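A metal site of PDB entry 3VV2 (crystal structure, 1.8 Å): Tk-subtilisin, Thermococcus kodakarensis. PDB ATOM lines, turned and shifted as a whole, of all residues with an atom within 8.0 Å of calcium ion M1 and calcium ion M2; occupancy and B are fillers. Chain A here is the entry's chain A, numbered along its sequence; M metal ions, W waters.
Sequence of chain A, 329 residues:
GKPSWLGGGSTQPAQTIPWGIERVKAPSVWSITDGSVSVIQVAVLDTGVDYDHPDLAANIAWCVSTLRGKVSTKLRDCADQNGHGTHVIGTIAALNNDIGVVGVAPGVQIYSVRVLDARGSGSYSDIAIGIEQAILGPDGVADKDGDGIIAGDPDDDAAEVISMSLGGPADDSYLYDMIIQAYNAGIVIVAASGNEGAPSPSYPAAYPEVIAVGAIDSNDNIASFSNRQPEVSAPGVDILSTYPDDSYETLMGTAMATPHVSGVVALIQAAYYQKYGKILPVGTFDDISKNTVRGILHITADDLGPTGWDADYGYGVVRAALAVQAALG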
ATOM      1  N   VAL A 141      22.850  -9.902  18.842  1.00  0.00           N
ATOM      2  CA  VAL A 141      22.022  -8.917  18.163  1.00  0.00           C
ATOM      3  C   VAL A 141      21.044  -9.666  17.214  1.00  0.00           C
ATOM      4  O   VAL A 141      21.468 -10.516  16.409  1.00  0.00           O
ATOM      5  CB  VAL A 141      22.910  -7.870  17.386  1.00  0.00           C
ATOM      6  CG1 VAL A 141      22.056  -6.735  16.765  1.00  0.00           C
ATOM      7  CG2 VAL A 141      24.044  -7.315  18.306  1.00  0.00           C
ATOM      8  N   ALA A 142      19.768  -9.356  17.365  1.00  0.00           N
ATOM      9  CA  ALA A 142      18.711  -9.956  16.590  1.00  0.00           C
ATOM     10  C   ALA A 142      18.857  -9.586  15.103  1.00  0.00           C
ATOM     11  O   ALA A 142      19.064 -10.480  14.254  1.00  0.00           O
ATOM     12  CB  ALA A 142      17.389  -9.474  17.144  1.00  0.00           C
ATOM     13  N   ASP A 143      18.902  -8.277  14.814  1.00  0.00           N
ATOM     14  CA  ASP A 143      18.867  -7.767  13.435  1.00  0.00           C
ATOM     15  C   ASP A 143      19.977  -6.725  13.220  1.00  0.00           C
ATOM     16  O   ASP A 143      19.703  -5.497  13.331  1.00  0.00           O
ATOM     17  CB  ASP A 143      17.486  -7.113  13.222  1.00  0.00           C
ATOM     18  CG  ASP A 143      17.293  -6.558  11.789  1.00  0.00           C
ATOM     19  OD1 ASP A 143      18.088  -6.855  10.920  1.00  0.00           O
ATOM     20  OD2 ASP A 143      16.303  -5.902  11.534  1.00  0.00           O
ATOM     21  N   LYS A 144      21.196  -7.174  12.912  1.00  0.00           N
ATOM     22  CA  LYS A 144      22.372  -6.300  12.948  1.00  0.00           C
ATOM     23  C   LYS A 144      22.324  -5.173  11.896  1.00  0.00           C
ATOM     24  O   LYS A 144      22.775  -4.051  12.172  1.00  0.00           O
ATOM     25  CB  LYS A 144      23.598  -7.126  12.625  1.00  0.00           C
ATOM     26  CG  LYS A 144      24.620  -7.131  13.703  1.00  0.00           C
ATOM     27  CD  LYS A 144      25.654  -8.216  13.382  1.00  0.00           C
ATOM     28  CE  LYS A 144      26.371  -7.941  12.064  1.00  0.00           C
ATOM     29  NZ  LYS A 144      26.670  -9.230  11.382  1.00  0.00           N
ATOM     30  N   ASP A 145      21.753  -5.444  10.738  1.00  0.00           N
ATOM     31  CA  ASP A 145      21.687  -4.455   9.701  1.00  0.00           C
ATOM     32  C   ASP A 145      20.372  -3.675   9.638  1.00  0.00           C
ATOM     33  O   ASP A 145      20.212  -2.806   8.817  1.00  0.00           O
ATOM     34  CB  ASP A 145      22.062  -5.053   8.363  1.00  0.00           C
ATOM     35  CG  ASP A 145      21.112  -6.137   7.920  1.00  0.00           C
ATOM     36  OD1 ASP A 145      21.351  -6.703   6.844  1.00  0.00           O
ATOM     37  OD2 ASP A 145      20.119  -6.489   8.560  1.00  0.00           O
ATOM     38  N   GLY A 146      19.443  -3.978  10.526  1.00  0.00           N
ATOM     39  CA  GLY A 146      18.230  -3.154  10.676  1.00  0.00           C
ATOM     40  C   GLY A 146      17.204  -3.283   9.593  1.00  0.00           C
ATOM     41  O   GLY A 146      16.247  -2.452   9.493  1.00  0.00           O
ATOM     42  N   ASP A 147      17.352  -4.305   8.771  1.00  0.00           N
ATOM     43  CA  ASP A 147      16.387  -4.485   7.646  1.00  0.00           C
ATOM     44  C   ASP A 147      15.100  -5.268   7.946  1.00  0.00           C
ATOM     45  O   ASP A 147      14.246  -5.380   7.063  1.00  0.00           O
ATOM     46  CB  ASP A 147      17.044  -5.048   6.387  1.00  0.00           C
ATOM     47  CG  ASP A 147      17.697  -6.433   6.625  1.00  0.00           C
ATOM     48  OD1 ASP A 147      17.484  -7.145   7.655  1.00  0.00           O
ATOM     49  OD2 ASP A 147      18.478  -6.798   5.767  1.00  0.00           O
ATOM     50  N   GLY A 148      14.924  -5.749   9.163  1.00  0.00           N
ATOM     51  CA  GLY A 148      13.667  -6.500   9.502  1.00  0.00           C
ATOM     52  C   GLY A 148      13.742  -7.970   9.120  1.00  0.00           C
ATOM     53  O   GLY A 148      12.891  -8.753   9.416  1.00  0.00           O
ATOM     54  N   ILE A 149      14.805  -8.380   8.419  1.00  0.00           N
ATOM     55  CA  ILE A 149      14.933  -9.764   8.059  1.00  0.00           C
ATOM     56  C   ILE A 149      15.847 -10.356   9.147  1.00  0.00           C
ATOM     57  O   ILE A 149      16.906  -9.820   9.368  1.00  0.00           O
ATOM     58  CB  ILE A 149      15.620  -9.911   6.658  1.00  0.00           C
ATOM     59  CG1 ILE A 149      15.087  -8.848   5.647  1.00  0.00           C
ATOM     60  CG2 ILE A 149      15.537 -11.371   6.137  1.00  0.00           C
ATOM     61  CD1 ILE A 149      15.260  -9.229   4.172  1.00  0.00           C
ATOM     62  N   ILE A 150      15.417 -11.396   9.808  1.00  0.00           N
ATOM     63  CA  ILE A 150      16.212 -12.037  10.825  1.00  0.00           C
ATOM     64  C   ILE A 150      16.472 -13.504  10.451  1.00  0.00           C
ATOM     65  O   ILE A 150      17.556 -13.851  10.081  1.00  0.00           O
ATOM     66  CB  ILE A 150      15.601 -11.863  12.233  1.00  0.00           C
ATOM     67  CG1 ILE A 150      15.536 -10.395  12.616  1.00  0.00           C
ATOM     68  CG2 ILE A 150      16.427 -12.602  13.264  1.00  0.00           C
ATOM     69  CD1 ILE A 150      14.441 -10.071  13.506  1.00  0.00           C
ATOM     70  N   ALA A 151      15.465 -14.351  10.477  1.00  0.00           N
ATOM     71  CA  ALA A 151      15.701 -15.732  10.092  1.00  0.00           C
ATOM     72  C   ALA A 151      15.820 -15.536   8.585  1.00  0.00           C
ATOM     73  O   ALA A 151      15.092 -14.703   7.993  1.00  0.00           O
ATOM     74  CB  ALA A 151      14.460 -16.607  10.449  1.00  0.00           C
ATOM     75  N   GLY A 152      16.755 -16.265   7.980  1.00  0.00           N
ATOM     76  CA  GLY A 152      17.010 -16.161   6.533  1.00  0.00           C
ATOM     77  C   GLY A 152      17.866 -15.011   6.019  1.00  0.00           C
ATOM     78  O   GLY A 152      18.192 -14.955   4.809  1.00  0.00           O
ATOM     79  N   ASP A 153      18.231 -14.081   6.888  1.00  0.00           N
ATOM     80  CA  ASP A 153      19.190 -13.052   6.529  1.00  0.00           C
ATOM     81  C   ASP A 153      20.601 -13.570   6.667  1.00  0.00           C
ATOM     82  O   ASP A 153      21.037 -13.883   7.758  1.00  0.00           O
ATOM     83  CB  ASP A 153      18.985 -11.807   7.379  1.00  0.00           C
ATOM     84  CG  ASP A 153      19.791 -10.621   6.892  1.00  0.00           C
ATOM     85  OD1 ASP A 153      19.476  -9.492   7.284  1.00  0.00           O
ATOM     86  OD2 ASP A 153      20.744 -10.738   6.124  1.00  0.00           O
ATOM     87  N   PRO A 154      21.327 -13.695   5.566  1.00  0.00           N
ATOM     88  CA  PRO A 154      22.695 -14.215   5.760  1.00  0.00           C
ATOM     89  C   PRO A 154      23.650 -13.338   6.576  1.00  0.00           C
ATOM     90  O   PRO A 154      24.679 -13.867   7.019  1.00  0.00           O
ATOM     91  CB  PRO A 154      23.231 -14.414   4.346  1.00  0.00           C
ATOM     92  CG  PRO A 154      22.346 -13.516   3.448  1.00  0.00           C
ATOM     93  CD  PRO A 154      21.021 -13.340   4.156  1.00  0.00           C
ATOM     94  N   ASP A 155      23.307 -12.060   6.770  1.00  0.00           N
ATOM     95  CA  ASP A 155      24.116 -11.093   7.566  1.00  0.00           C
ATOM     96  C   ASP A 155      23.856 -11.331   9.070  1.00  0.00           C
ATOM     97  O   ASP A 155      24.696 -11.007   9.961  1.00  0.00           O
ATOM     98  CB  ASP A 155      23.835  -9.612   7.201  1.00  0.00           C
ATOM     99  CG  ASP A 155      24.729  -8.680   7.955  1.00  0.00           C
ATOM    100  OD1 ASP A 155      25.953  -8.902   7.891  1.00  0.00           O
ATOM    101  OD2 ASP A 155      24.265  -7.782   8.692  1.00  0.00           O
ATOM    102  N   ASP A 156      22.726 -11.940   9.370  1.00  0.00           N
ATOM    103  CA  ASP A 156      22.500 -12.326  10.775  1.00  0.00           C
ATOM    104  C   ASP A 156      22.827 -13.812  11.107  1.00  0.00           C
ATOM    105  O   ASP A 156      23.120 -14.616  10.222  1.00  0.00           O
ATOM    106  CB  ASP A 156      21.078 -11.997  11.221  1.00  0.00           C
ATOM    107  CG  ASP A 156      20.817 -10.484  11.317  1.00  0.00           C
ATOM    108  OD1 ASP A 156      21.566  -9.805  12.049  1.00  0.00           O
ATOM    109  OD2 ASP A 156      19.872  -9.986  10.677  1.00  0.00           O
ATOM    110  N   ASP A 157      22.770 -14.143  12.384  1.00  0.00           N
ATOM    111  CA  ASP A 157      23.067 -15.498  12.839  1.00  0.00           C
ATOM    112  C   ASP A 157      21.919 -16.081  13.636  1.00  0.00           C
ATOM    113  O   ASP A 157      22.115 -16.967  14.465  1.00  0.00           O
ATOM    114  CB  ASP A 157      24.354 -15.509  13.670  1.00  0.00           C
ATOM    115  CG  ASP A 157      24.309 -14.535  14.828  1.00  0.00           C
ATOM    116  OD1 ASP A 157      25.337 -14.399  15.527  1.00  0.00           O
ATOM    117  OD2 ASP A 157      23.257 -13.902  15.032  1.00  0.00           O
HETATM  118 CA    CA M   1      18.870  -8.327   9.225  1.00  0.00          CA
HETATM  119 CA    CA M   2      20.068  -8.002   5.938  1.00  0.00          CA
HETATM  120  O   HOH W   1      21.634  -8.394   9.636  1.00  0.00           O
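Calcium ion M2 is bound by OD2 of Asp 147 (2.0 Å), OD1 of Asp 145 (2.0 Å), OD1 of Asp 153 (2.1 Å) and OD2 of Asp 153 (2.8 Å). Calcium ion M2 has four donor atoms within binding distance. Slightly farther from calcium ion M2 lies the side-chain carboxylate (OD2) of Asp 145 (3.0 Å).
Calcium ion M1 is bound by the side-chain carboxylate (OD2) of Asp 145 (2.3 Å), the side-chain carboxylate (OD1) of Asp 153 (2.3 Å), the side-chain carboxylate (OD1) of Asp 143 (2.4 Å), the side-chain carboxylate (OD1) of Asp 147 (2.4 Å), the side-chain carboxylate (OD2) of Asp 156 (2.4 Å), the backbone carbonyl oxygen (O) of Ile 149 (2.5 Å) and water W1 (2.8 Å). Calcium ion M1 has seven donor atoms within binding distance.
Within 4 Å of calcium ion M1: Asp 143, Asp 145, Asp 147, Ile 149, Asp 153 and Asp 156. Along chain A the residues within 4 Å of calcium ion M1 span positions 143 to 156. The nearest printed residue that does not touch calcium ion M1 is Lys 144 (4.5 Å).
N of Lys 144 sits at hydrogen-bond distance from OD1 of Asp 156, 2.8 Å away. The backbone NH (N) of Gly 148 is in hydrogen-bond range of the side-chain carboxylate (OD2) of Asp 143, at 2.7 Å. The side-chain carboxylate (OD2) of Asp 153 lies close to the backbone NH (N) of Asp 155 (3.0 Å). The side-chain carboxylate of Asp 143 lies close to the backbone NH of Gly 146, 3.2 Å away.
Three residues have an atom within 4 Å of calcium ion M2: Asp 145, Asp 147 and Asp 153.
Water W1 lies within hydrogen-bond range of OD1 of Asp 156 (2.8 Å), OD2 of Asp 155 (2.9 Å) and N of Asp 145 (3.2 Å).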
